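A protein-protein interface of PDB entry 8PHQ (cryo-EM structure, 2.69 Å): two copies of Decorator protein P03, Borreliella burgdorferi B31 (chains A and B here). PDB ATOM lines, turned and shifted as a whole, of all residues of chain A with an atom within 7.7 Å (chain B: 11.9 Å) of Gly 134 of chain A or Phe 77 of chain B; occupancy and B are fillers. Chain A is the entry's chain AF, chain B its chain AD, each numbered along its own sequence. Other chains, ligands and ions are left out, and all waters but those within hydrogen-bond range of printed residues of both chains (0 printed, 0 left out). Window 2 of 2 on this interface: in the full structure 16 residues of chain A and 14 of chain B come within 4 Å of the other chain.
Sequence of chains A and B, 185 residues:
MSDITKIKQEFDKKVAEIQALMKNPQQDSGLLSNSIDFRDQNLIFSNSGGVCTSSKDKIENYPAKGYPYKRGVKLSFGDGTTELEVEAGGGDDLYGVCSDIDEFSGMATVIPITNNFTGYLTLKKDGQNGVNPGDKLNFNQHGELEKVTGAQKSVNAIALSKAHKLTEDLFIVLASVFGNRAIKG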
ATOM      1  N   VAL A 131     -16.476  29.794  14.406  1.00  0.00           N
ATOM      2  CA  VAL A 131     -16.523  28.467  15.004  1.00  0.00           C
ATOM      3  C   VAL A 131     -15.820  28.477  16.357  1.00  0.00           C
ATOM      4  O   VAL A 131     -14.634  28.787  16.451  1.00  0.00           O
ATOM      5  CB  VAL A 131     -15.904  27.416  14.069  1.00  0.00           C
ATOM      6  CG1 VAL A 131     -15.787  26.078  14.778  1.00  0.00           C
ATOM      7  CG2 VAL A 131     -16.735  27.280  12.805  1.00  0.00           C
ATOM      8  N   ASN A 132     -16.563  28.131  17.397  1.00  0.00           N
ATOM      9  CA  ASN A 132     -16.099  28.138  18.775  1.00  0.00           C
ATOM     10  C   ASN A 132     -16.378  26.785  19.405  1.00  0.00           C
ATOM     11  O   ASN A 132     -17.228  26.030  18.920  1.00  0.00           O
ATOM     12  CB  ASN A 132     -16.792  29.248  19.581  1.00  0.00           C
ATOM     13  CG  ASN A 132     -16.568  30.625  18.986  1.00  0.00           C
ATOM     14  OD1 ASN A 132     -15.431  31.061  18.813  1.00  0.00           O
ATOM     15  ND2 ASN A 132     -17.655  31.316  18.670  1.00  0.00           N
ATOM     16  N   PRO A 133     -15.663  26.436  20.477  1.00  0.00           N
ATOM     17  CA  PRO A 133     -15.909  25.148  21.136  1.00  0.00           C
ATOM     18  C   PRO A 133     -17.356  25.012  21.585  1.00  0.00           C
ATOM     19  O   PRO A 133     -17.963  25.957  22.090  1.00  0.00           O
ATOM     20  CB  PRO A 133     -14.952  25.179  22.331  1.00  0.00           C
ATOM     21  CG  PRO A 133     -13.835  26.038  21.871  1.00  0.00           C
ATOM     22  CD  PRO A 133     -14.473  27.109  21.028  1.00  0.00           C
ATOM     23  N   GLY A 134     -17.903  23.813  21.396  1.00  0.00           N
ATOM     24  CA  GLY A 134     -19.284  23.526  21.696  1.00  0.00           C
ATOM     25  C   GLY A 134     -20.222  23.644  20.512  1.00  0.00           C
ATOM     26  O   GLY A 134     -21.361  23.171  20.593  1.00  0.00           O
ATOM     27  N   ASP A 135     -19.774  24.260  19.422  1.00  0.00           N
ATOM     28  CA  ASP A 135     -20.612  24.403  18.241  1.00  0.00           C
ATOM     29  C   ASP A 135     -20.867  23.049  17.593  1.00  0.00           C
ATOM     30  O   ASP A 135     -19.973  22.205  17.504  1.00  0.00           O
ATOM     31  CB  ASP A 135     -19.956  25.348  17.235  1.00  0.00           C
ATOM     32  CG  ASP A 135     -19.974  26.790  17.694  1.00  0.00           C
ATOM     33  OD1 ASP A 135     -20.520  27.059  18.784  1.00  0.00           O
ATOM     34  OD2 ASP A 135     -19.438  27.654  16.969  1.00  0.00           O
ATOM     35  N   LYS A 136     -22.100  22.847  17.136  1.00  0.00           N
ATOM     36  CA  LYS A 136     -22.486  21.614  16.464  1.00  0.00           C
ATOM     37  C   LYS A 136     -22.166  21.725  14.980  1.00  0.00           C
ATOM     38  O   LYS A 136     -22.503  22.725  14.339  1.00  0.00           O
ATOM     39  CB  LYS A 136     -23.972  21.331  16.678  1.00  0.00           C
ATOM     40  CG  LYS A 136     -24.343  21.122  18.136  1.00  0.00           C
ATOM     41  CD  LYS A 136     -25.788  20.686  18.288  1.00  0.00           C
ATOM     42  CE  LYS A 136     -26.137  20.448  19.746  1.00  0.00           C
ATOM     43  NZ  LYS A 136     -27.521  19.924  19.908  1.00  0.00           N
ATOM     44  N   LEU A 137     -21.520  20.696  14.439  1.00  0.00           N
ATOM     45  CA  LEU A 137     -21.011  20.716  13.078  1.00  0.00           C
ATOM     46  C   LEU A 137     -21.653  19.612  12.249  1.00  0.00           C
ATOM     47  O   LEU A 137     -22.241  18.665  12.776  1.00  0.00           O
ATOM     48  CB  LEU A 137     -19.487  20.556  13.057  1.00  0.00           C
ATOM     49  CG  LEU A 137     -18.692  21.532  13.924  1.00  0.00           C
ATOM     50  CD1 LEU A 137     -17.203  21.264  13.794  1.00  0.00           C
ATOM     51  CD2 LEU A 137     -19.015  22.964  13.546  1.00  0.00           C
ATOM     52  N   LYS A 147     -20.598  24.775  10.416  1.00  0.00           N
ATOM     53  CA  LYS A 147     -21.495  25.015  11.537  1.00  0.00           C
ATOM     54  C   LYS A 147     -22.942  24.782  11.120  1.00  0.00           C
ATOM     55  O   LYS A 147     -23.372  25.223  10.051  1.00  0.00           O
ATOM     56  CB  LYS A 147     -21.316  26.439  12.057  1.00  0.00           C
ATOM     57  CG  LYS A 147     -22.096  26.750  13.321  1.00  0.00           C
ATOM     58  CD  LYS A 147     -21.759  28.138  13.839  1.00  0.00           C
ATOM     59  CE  LYS A 147     -22.565  28.478  15.078  1.00  0.00           C
ATOM     60  NZ  LYS A 147     -22.245  29.839  15.588  1.00  0.00           N
ATOM     61  N   ALA A 157     -21.333  15.868  15.366  1.00  0.00           N
ATOM     62  CA  ALA A 157     -19.961  16.351  15.402  1.00  0.00           C
ATOM     63  C   ALA A 157     -19.927  17.640  16.206  1.00  0.00           C
ATOM     64  O   ALA A 157     -20.728  18.547  15.960  1.00  0.00           O
ATOM     65  CB  ALA A 157     -19.412  16.587  13.993  1.00  0.00           C
ATOM     66  N   ILE A 158     -19.007  17.716  17.164  1.00  0.00           N
ATOM     67  CA  ILE A 158     -18.890  18.865  18.054  1.00  0.00           C
ATOM     68  C   ILE A 158     -17.448  19.351  18.041  1.00  0.00           C
ATOM     69  O   ILE A 158     -16.518  18.553  18.205  1.00  0.00           O
ATOM     70  CB  ILE A 158     -19.337  18.523  19.487  1.00  0.00           C
ATOM     71  CG1 ILE A 158     -20.828  18.181  19.508  1.00  0.00           C
ATOM     72  CG2 ILE A 158     -19.044  19.676  20.431  1.00  0.00           C
ATOM     73  CD1 ILE A 158     -21.374  17.910  20.890  1.00  0.00           C
ATOM     74  N   ALA A 159     -17.265  20.655  17.847  1.00  0.00           N
ATOM     75  CA  ALA A 159     -15.935  21.246  17.831  1.00  0.00           C
ATOM     76  C   ALA A 159     -15.422  21.458  19.248  1.00  0.00           C
ATOM     77  O   ALA A 159     -16.139  21.964  20.116  1.00  0.00           O
ATOM     78  CB  ALA A 159     -15.950  22.574  17.076  1.00  0.00           C
ATOM     79  N   LEU A 160     -14.169  21.071  19.477  1.00  0.00           N
ATOM     80  CA  LEU A 160     -13.533  21.188  20.779  1.00  0.00           C
ATOM     81  C   LEU A 160     -12.538  22.337  20.852  1.00  0.00           C
ATOM     82  O   LEU A 160     -11.872  22.494  21.880  1.00  0.00           O
ATOM     83  CB  LEU A 160     -12.820  19.879  21.133  1.00  0.00           C
ATOM     84  CG  LEU A 160     -13.653  18.597  21.113  1.00  0.00           C
ATOM     85  CD1 LEU A 160     -12.835  17.439  21.656  1.00  0.00           C
ATOM     86  CD2 LEU A 160     -14.937  18.766  21.899  1.00  0.00           C
ATOM     87  N   SER A 161     -12.412  23.133  19.797  1.00  0.00           N
ATOM     88  CA  SER A 161     -11.476  24.249  19.775  1.00  0.00           C
ATOM     89  C   SER A 161     -11.933  25.232  18.704  1.00  0.00           C
ATOM     90  O   SER A 161     -13.019  25.095  18.133  1.00  0.00           O
ATOM     91  CB  SER A 161     -10.044  23.766  19.528  1.00  0.00           C
ATOM     92  OG  SER A 161      -9.858  23.397  18.173  1.00  0.00           O
ATOM     93  N   LEU A 174     -10.222  20.876  15.801  1.00  0.00           N
ATOM     94  CA  LEU A 174     -10.371  19.671  16.602  1.00  0.00           C
ATOM     95  C   LEU A 174     -11.850  19.377  16.791  1.00  0.00           C
ATOM     96  O   LEU A 174     -12.617  20.251  17.200  1.00  0.00           O
ATOM     97  CB  LEU A 174      -9.686  19.842  17.955  1.00  0.00           C
ATOM     98  CG  LEU A 174      -9.767  18.658  18.917  1.00  0.00           C
ATOM     99  CD1 LEU A 174      -8.978  17.482  18.379  1.00  0.00           C
ATOM    100  CD2 LEU A 174      -9.264  19.059  20.289  1.00  0.00           C
ATOM    101  N   SER A 176     -14.983  16.143  17.679  1.00  0.00           N
ATOM    102  CA  SER A 176     -15.412  14.820  18.109  1.00  0.00           C
ATOM    103  C   SER A 176     -16.641  14.433  17.301  1.00  0.00           C
ATOM    104  O   SER A 176     -17.661  15.130  17.344  1.00  0.00           O
ATOM    105  CB  SER A 176     -15.722  14.798  19.604  1.00  0.00           C
ATOM    106  OG  SER A 176     -14.558  15.056  20.366  1.00  0.00           O
ATOM    107  N   TYR B  62     -13.205  10.780  31.725  1.00  0.00           N
ATOM    108  CA  TYR B  62     -13.256  12.231  31.663  1.00  0.00           C
ATOM    109  C   TYR B  62     -13.368  12.824  33.058  1.00  0.00           C
ATOM    110  O   TYR B  62     -13.850  12.163  33.981  1.00  0.00           O
ATOM    111  CB  TYR B  62     -14.440  12.709  30.812  1.00  0.00           C
ATOM    112  CG  TYR B  62     -14.309  12.394  29.341  1.00  0.00           C
ATOM    113  CD1 TYR B  62     -13.275  12.933  28.589  1.00  0.00           C
ATOM    114  CD2 TYR B  62     -15.219  11.564  28.703  1.00  0.00           C
ATOM    115  CE1 TYR B  62     -13.149  12.652  27.245  1.00  0.00           C
ATOM    116  CE2 TYR B  62     -15.100  11.277  27.358  1.00  0.00           C
ATOM    117  CZ  TYR B  62     -14.064  11.823  26.634  1.00  0.00           C
ATOM    118  OH  TYR B  62     -13.942  11.540  25.293  1.00  0.00           O
ATOM    119  N   PRO B  63     -12.917  14.061  33.246  1.00  0.00           N
ATOM    120  CA  PRO B  63     -13.198  14.754  34.508  1.00  0.00           C
ATOM    121  C   PRO B  63     -14.699  14.894  34.710  1.00  0.00           C
ATOM    122  O   PRO B  63     -15.451  15.150  33.768  1.00  0.00           O
ATOM    123  CB  PRO B  63     -12.517  16.114  34.327  1.00  0.00           C
ATOM    124  CG  PRO B  63     -11.476  15.881  33.285  1.00  0.00           C
ATOM    125  CD  PRO B  63     -12.052  14.858  32.359  1.00  0.00           C
ATOM    126  N   ALA B  64     -15.133  14.722  35.953  1.00  0.00           N
ATOM    127  CA  ALA B  64     -16.548  14.667  36.279  1.00  0.00           C
ATOM    128  C   ALA B  64     -16.987  15.927  37.011  1.00  0.00           C
ATOM    129  O   ALA B  64     -16.236  16.505  37.801  1.00  0.00           O
ATOM    130  CB  ALA B  64     -16.867  13.437  37.133  1.00  0.00           C
ATOM    131  N   LYS B  65     -18.218  16.345  36.733  1.00  0.00           N
ATOM    132  CA  LYS B  65     -18.866  17.447  37.429  1.00  0.00           C
ATOM    133  C   LYS B  65     -20.147  16.923  38.060  1.00  0.00           C
ATOM    134  O   LYS B  65     -20.948  16.266  37.388  1.00  0.00           O
ATOM    135  CB  LYS B  65     -19.177  18.601  36.474  1.00  0.00           C
ATOM    136  CG  LYS B  65     -19.965  19.734  37.106  1.00  0.00           C
ATOM    137  CD  LYS B  65     -20.281  20.816  36.089  1.00  0.00           C
ATOM    138  CE  LYS B  65     -21.176  21.891  36.682  1.00  0.00           C
ATOM    139  NZ  LYS B  65     -21.532  22.932  35.677  1.00  0.00           N
ATOM    140  N   VAL B  73     -24.611  11.011  30.087  1.00  0.00           N
ATOM    141  CA  VAL B  73     -23.755  12.169  30.294  1.00  0.00           C
ATOM    142  C   VAL B  73     -23.653  12.978  29.010  1.00  0.00           C
ATOM    143  O   VAL B  73     -23.853  12.472  27.904  1.00  0.00           O
ATOM    144  CB  VAL B  73     -22.347  11.770  30.779  1.00  0.00           C
ATOM    145  CG1 VAL B  73     -22.418  11.160  32.163  1.00  0.00           C
ATOM    146  CG2 VAL B  73     -21.705  10.805  29.799  1.00  0.00           C
ATOM    147  N   LYS B  74     -23.338  14.257  29.182  1.00  0.00           N
ATOM    148  CA  LYS B  74     -23.091  15.177  28.086  1.00  0.00           C
ATOM    149  C   LYS B  74     -21.777  15.901  28.340  1.00  0.00           C
ATOM    150  O   LYS B  74     -21.306  16.001  29.479  1.00  0.00           O
ATOM    151  CB  LYS B  74     -24.218  16.207  27.931  1.00  0.00           C
ATOM    152  CG  LYS B  74     -24.457  17.049  29.169  1.00  0.00           C
ATOM    153  CD  LYS B  74     -25.621  18.003  28.978  1.00  0.00           C
ATOM    154  CE  LYS B  74     -25.922  18.760  30.261  1.00  0.00           C
ATOM    155  NZ  LYS B  74     -27.058  19.709  30.099  1.00  0.00           N
ATOM    156  N   LEU B  75     -21.196  16.409  27.256  1.00  0.00           N
ATOM    157  CA  LEU B  75     -19.973  17.195  27.335  1.00  0.00           C
ATOM    158  C   LEU B  75     -20.302  18.635  27.702  1.00  0.00           C
ATOM    159  O   LEU B  75     -21.178  19.257  27.092  1.00  0.00           O
ATOM    160  CB  LEU B  75     -19.225  17.155  26.002  1.00  0.00           C
ATOM    161  CG  LEU B  75     -18.600  15.829  25.568  1.00  0.00           C
ATOM    162  CD1 LEU B  75     -17.822  16.008  24.274  1.00  0.00           C
ATOM    163  CD2 LEU B  75     -17.701  15.278  26.654  1.00  0.00           C
ATOM    164  N   SER B  76     -19.601  19.164  28.700  1.00  0.00           N
ATOM    165  CA  SER B  76     -19.752  20.540  29.142  1.00  0.00           C
ATOM    166  C   SER B  76     -18.401  21.234  29.067  1.00  0.00           C
ATOM    167  O   SER B  76     -17.386  20.690  29.523  1.00  0.00           O
ATOM    168  CB  SER B  76     -20.315  20.604  30.565  1.00  0.00           C
ATOM    169  OG  SER B  76     -19.399  20.069  31.501  1.00  0.00           O
ATOM    170  N   PHE B  77     -18.398  22.429  28.483  1.00  0.00           N
ATOM    171  CA  PHE B  77     -17.193  23.214  28.264  1.00  0.00           C
ATOM    172  C   PHE B  77     -17.219  24.436  29.170  1.00  0.00           C
ATOM    173  O   PHE B  77     -18.237  25.132  29.250  1.00  0.00           O
ATOM    174  CB  PHE B  77     -17.069  23.660  26.802  1.00  0.00           C
ATOM    175  CG  PHE B  77     -17.291  22.561  25.799  1.00  0.00           C
ATOM    176  CD1 PHE B  77     -18.565  22.085  25.528  1.00  0.00           C
ATOM    177  CD2 PHE B  77     -16.220  22.000  25.128  1.00  0.00           C
ATOM    178  CE1 PHE B  77     -18.763  21.077  24.609  1.00  0.00           C
ATOM    179  CE2 PHE B  77     -16.413  20.991  24.209  1.00  0.00           C
ATOM    180  CZ  PHE B  77     -17.686  20.529  23.948  1.00  0.00           C
ATOM    181  N   GLY B  78     -16.104  24.697  29.841  1.00  0.00           N
ATOM    182  CA  GLY B  78     -15.971  25.873  30.672  1.00  0.00           C
ATOM    183  C   GLY B  78     -15.575  27.085  29.854  1.00  0.00           C
ATOM    184  O   GLY B  78     -15.782  27.149  28.639  1.00  0.00           O
ATOM    185  N   ASP B  79     -15.002  28.072  30.544  1.00  0.00           N
ATOM    186  CA  ASP B  79     -14.493  29.250  29.850  1.00  0.00           C
ATOM    187  C   ASP B  79     -13.341  28.894  28.921  1.00  0.00           C
ATOM    188  O   ASP B  79     -13.195  29.498  27.852  1.00  0.00           O
ATOM    189  CB  ASP B  79     -14.053  30.309  30.861  1.00  0.00           C
ATOM    190  CG  ASP B  79     -13.182  31.381  30.236  1.00  0.00           C
ATOM    191  OD1 ASP B  79     -13.669  32.086  29.328  1.00  0.00           O
ATOM    192  OD2 ASP B  79     -12.012  31.516  30.652  1.00  0.00           O
ATOM    193  N   GLY B  80     -12.524  27.918  29.304  1.00  0.00           N
ATOM    194  CA  GLY B  80     -11.374  27.529  28.514  1.00  0.00           C
ATOM    195  C   GLY B  80     -10.138  27.348  29.368  1.00  0.00           C
ATOM    196  O   GLY B  80      -9.136  26.787  28.914  1.00  0.00           O
ATOM    197  N   THR B  81     -10.202  27.825  30.613  1.00  0.00           N
ATOM    198  CA  THR B  81      -9.081  27.657  31.531  1.00  0.00           C
ATOM    199  C   THR B  81      -8.835  26.185  31.836  1.00  0.00           C
ATOM    200  O   THR B  81      -7.684  25.740  31.906  1.00  0.00           O
ATOM    201  CB  THR B  81      -9.337  28.435  32.821  1.00  0.00           C
ATOM    202  OG1 THR B  81      -9.675  29.791  32.505  1.00  0.00           O
ATOM    203  CG2 THR B  81      -8.099  28.424  33.706  1.00  0.00           C
ATOM    204  N   THR B  82      -9.903  25.414  32.015  1.00  0.00           N
ATOM    205  CA  THR B  82      -9.812  23.994  32.306  1.00  0.00           C
ATOM    206  C   THR B  82     -10.422  23.197  31.160  1.00  0.00           C
ATOM    207  O   THR B  82     -11.241  23.702  30.388  1.00  0.00           O
ATOM    208  CB  THR B  82     -10.521  23.643  33.620  1.00  0.00           C
ATOM    209  OG1 THR B  82     -11.884  24.079  33.562  1.00  0.00           O
ATOM    210  CG2 THR B  82      -9.829  24.316  34.795  1.00  0.00           C
ATOM    211  N   GLU B  83     -10.009  21.936  31.062  1.00  0.00           N
ATOM    212  CA  GLU B  83     -10.450  21.076  29.977  1.00  0.00           C
ATOM    213  C   GLU B  83     -11.936  20.752  30.114  1.00  0.00           C
ATOM    214  O   GLU B  83     -12.554  20.943  31.165  1.00  0.00           O
ATOM    215  CB  GLU B  83      -9.627  19.790  29.951  1.00  0.00           C
ATOM    216  CG  GLU B  83      -9.549  19.084  31.292  1.00  0.00           C
ATOM    217  CD  GLU B  83      -8.673  17.849  31.250  1.00  0.00           C
ATOM    218  OE1 GLU B  83      -8.150  17.527  30.162  1.00  0.00           O
ATOM    219  OE2 GLU B  83      -8.505  17.200  32.302  1.00  0.00           O
ATOM    220  N   LEU B  84     -12.510  20.255  29.022  1.00  0.00           N
ATOM    221  CA  LEU B  84     -13.919  19.889  29.005  1.00  0.00           C
ATOM    222  C   LEU B  84     -14.187  18.738  29.967  1.00  0.00           C
ATOM    223  O   LEU B  84     -13.305  17.927  30.263  1.00  0.00           O
ATOM    224  CB  LEU B  84     -14.348  19.517  27.583  1.00  0.00           C
ATOM    225  CG  LEU B  84     -13.671  18.339  26.869  1.00  0.00           C
ATOM    226  CD1 LEU B  84     -14.288  16.986  27.221  1.00  0.00           C
ATOM    227  CD2 LEU B  84     -13.681  18.559  25.365  1.00  0.00           C
ATOM    228  N   GLU B  85     -15.422  18.671  30.459  1.00  0.00           N
ATOM    229  CA  GLU B  85     -15.799  17.648  31.425  1.00  0.00           C
ATOM    230  C   GLU B  85     -17.144  17.065  31.020  1.00  0.00           C
ATOM    231  O   GLU B  85     -17.733  17.457  30.012  1.00  0.00           O
ATOM    232  CB  GLU B  85     -15.823  18.225  32.844  1.00  0.00           C
ATOM    233  CG  GLU B  85     -16.682  19.460  32.987  1.00  0.00           C
ATOM    234  CD  GLU B  85     -16.766  19.944  34.414  1.00  0.00           C
ATOM    235  OE1 GLU B  85     -16.154  19.305  35.295  1.00  0.00           O
ATOM    236  OE2 GLU B  85     -17.441  20.965  34.657  1.00  0.00           O
ATOM    237  N   VAL B  86     -17.627  16.100  31.796  1.00  0.00           N
ATOM    238  CA  VAL B  86     -18.899  15.441  31.528  1.00  0.00           C
ATOM    239  C   VAL B  86     -19.824  15.648  32.718  1.00  0.00           C
ATOM    240  O   VAL B  86     -19.386  15.626  33.873  1.00  0.00           O
ATOM    241  CB  VAL B  86     -18.721  13.938  31.221  1.00  0.00           C
ATOM    242  CG1 VAL B  86     -17.886  13.752  29.969  1.00  0.00           C
ATOM    243  CG2 VAL B  86     -18.078  13.219  32.393  1.00  0.00           C
ATOM    244  N   GLU B  87     -21.103  15.872  32.430  1.00  0.00           N
ATOM    245  CA  GLU B  87     -22.096  16.032  33.483  1.00  0.00           C
ATOM    246  C   GLU B  87     -23.385  15.337  33.076  1.00  0.00           C
ATOM    247  O   GLU B  87     -23.661  15.142  31.891  1.00  0.00           O
ATOM    248  CB  GLU B  87     -22.363  17.509  33.799  1.00  0.00           C
ATOM    249  CG  GLU B  87     -22.824  18.329  32.611  1.00  0.00           C
ATOM    250  CD  GLU B  87     -23.000  19.793  32.957  1.00  0.00           C
ATOM    251  OE1 GLU B  87     -22.762  20.160  34.126  1.00  0.00           O
ATOM    252  OE2 GLU B  87     -23.375  20.577  32.060  1.00  0.00           O
ATOM    253  N   ALA B  88     -24.179  14.973  34.081  1.00  0.00           N
ATOM    254  CA  ALA B  88     -25.410  14.231  33.837  1.00  0.00           C
ATOM    255  C   ALA B  88     -26.346  15.019  32.930  1.00  0.00           C
ATOM    256  O   ALA B  88     -26.572  16.215  33.135  1.00  0.00           O
ATOM    257  CB  ALA B  88     -26.102  13.908  35.159  1.00  0.00           C
ATOM    258  N   ASP B  92     -30.953  15.690  23.250  1.00  0.00           N
ATOM    259  CA  ASP B  92     -30.202  15.887  22.019  1.00  0.00           C
ATOM    260  C   ASP B  92     -28.709  16.069  22.253  1.00  0.00           C
ATOM    261  O   ASP B  92     -27.942  16.062  21.284  1.00  0.00           O
ATOM    262  CB  ASP B  92     -30.749  17.100  21.262  1.00  0.00           C
ATOM    263  CG  ASP B  92     -32.262  17.116  21.207  1.00  0.00           C
ATOM    264  OD1 ASP B  92     -32.850  16.155  20.668  1.00  0.00           O
ATOM    265  OD2 ASP B  92     -32.866  18.090  21.707  1.00  0.00           O
ATOM    266  N   ASP B  93     -28.277  16.226  23.504  1.00  0.00           N
ATOM    267  CA  ASP B  93     -26.876  16.453  23.830  1.00  0.00           C
ATOM    268  C   ASP B  93     -26.212  15.219  24.429  1.00  0.00           C
ATOM    269  O   ASP B  93     -25.122  15.323  25.000  1.00  0.00           O
ATOM    270  CB  ASP B  93     -26.742  17.639  24.786  1.00  0.00           C
ATOM    271  CG  ASP B  93     -27.297  18.923  24.204  1.00  0.00           C
ATOM    272  OD1 ASP B  93     -27.775  18.900  23.052  1.00  0.00           O
ATOM    273  OD2 ASP B  93     -27.258  19.958  24.901  1.00  0.00           O
ATOM    274  N   LEU B  94     -26.842  14.053  24.310  1.00  0.00           N
ATOM    275  CA  LEU B  94     -26.298  12.845  24.915  1.00  0.00           C
ATOM    276  C   LEU B  94     -25.015  12.426  24.209  1.00  0.00           C
ATOM    277  O   LEU B  94     -24.981  12.292  22.983  1.00  0.00           O
ATOM    278  CB  LEU B  94     -27.325  11.717  24.858  1.00  0.00           C
ATOM    279  CG  LEU B  94     -26.915  10.421  25.556  1.00  0.00           C
ATOM    280  CD1 LEU B  94     -27.030  10.573  27.061  1.00  0.00           C
ATOM    281  CD2 LEU B  94     -27.758   9.260  25.064  1.00  0.00           C
ATOM    282  N   TYR B  95     -23.959  12.213  24.991  1.00  0.00           N
ATOM    283  CA  TYR B  95     -22.670  11.784  24.465  1.00  0.00           C
ATOM    284  C   TYR B  95     -22.336  10.336  24.782  1.00  0.00           C
ATOM    285  O   TYR B  95     -21.699   9.671  23.964  1.00  0.00           O
ATOM    286  CB  TYR B  95     -21.548  12.676  25.010  1.00  0.00           C
ATOM    287  CG  TYR B  95     -20.164  12.220  24.616  1.00  0.00           C
ATOM    288  CD1 TYR B  95     -19.766  12.217  23.287  1.00  0.00           C
ATOM    289  CD2 TYR B  95     -19.261  11.777  25.570  1.00  0.00           C
ATOM    290  CE1 TYR B  95     -18.503  11.794  22.922  1.00  0.00           C
ATOM    291  CE2 TYR B  95     -17.998  11.353  25.216  1.00  0.00           C
ATOM    292  CZ  TYR B  95     -17.624  11.363  23.890  1.00  0.00           C
ATOM    293  OH  TYR B  95     -16.366  10.940  23.531  1.00  0.00           O
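The side-chain carboxylate (OD1) of Asp 93 of chain B is in salt-bridge range of the side-chain amino group (NZ) of Lys 136 of chain A (3.3 Å).
The backbone carbonyl oxygen (O) of Leu 174 of chain A sits at hydrogen-bond distance from the backbone NH (N) of Leu 160 of chain A (2.9 Å). The backbone NH (N) of Gly 134 of chain A is in hydrogen-bond range of the backbone carbonyl oxygen (O) of Ala 159 of chain A, at 2.9 Å. The backbone carbonyl oxygen (O) of Ile 158 of chain A lies within hydrogen-bond range of the backbone NH (N) of Ser 176 of chain A (2.9 Å).
Among the printed residues, pairs that only touch across the chains: Gly 134 of chain A with Phe 77 of chain B, Ile 158 of chain A with Phe 77 of chain B, Leu 160 of chain A with Phe 77 of chain B and Leu 160 of chain A with Leu 84 of chain B.
Of chain B, only Phe 77 (3.8 Å) comes within 4 Å of Gly 134 of chain A. Phe 77 of chain B touches three residues of chain A. Asp 135 of chain A touches none of the printed residues of chain B. Lys 136 of chain A touches just one residue of chain B: Asp 93. Of chain B, only Phe 77 comes within 4 Å of Ile 158 of chain A. No residue of chain B comes within 4 Å of Ala 159 of chain A. Leu 160 of chain A touches just these residues of chain B: Phe 77 (3.5 Å) and Leu 84 (3.7 Å). No residue of chain A comes within 4 Å of Gly 78 of chain B. Printed residues of chain A within 4 Å of Asp 93 of chain B: Lys 136 (3.3 Å). Printed residues of chain A within 4 Å of Leu 84 of chain B: Leu 160. Leu 75 of chain B touches none of the printed residues of chain A. The nearest residue of chain A that does not touch Phe 77 of chain B is Ala 159 of chain A (4.2 Å). The nearest printed residue of chain A that does not touch Asp 93 of chain B is Ile 158 of chain A (6.1 Å).
Printed residues of chain B that touch a printed residue of chain A: Phe 77, Leu 84 and Asp 93. Printed residues of chain A that touch a printed residue of chain B: Gly 134, Lys 136, Ile 158 and Leu 160. Hydrophobic or aromatic side chains of chain A that line the printed part of chain B: Ile 158 and Leu 160. Among the printed residues, 5 pairs touch across the chains. Among the printed residues, Asp or Glu carboxylates within 4 Å of a Lys or Arg side-chain nitrogen of the other chain: Lys 136 of chain A with Asp 93 of chain B.
No position is printed for both chains.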
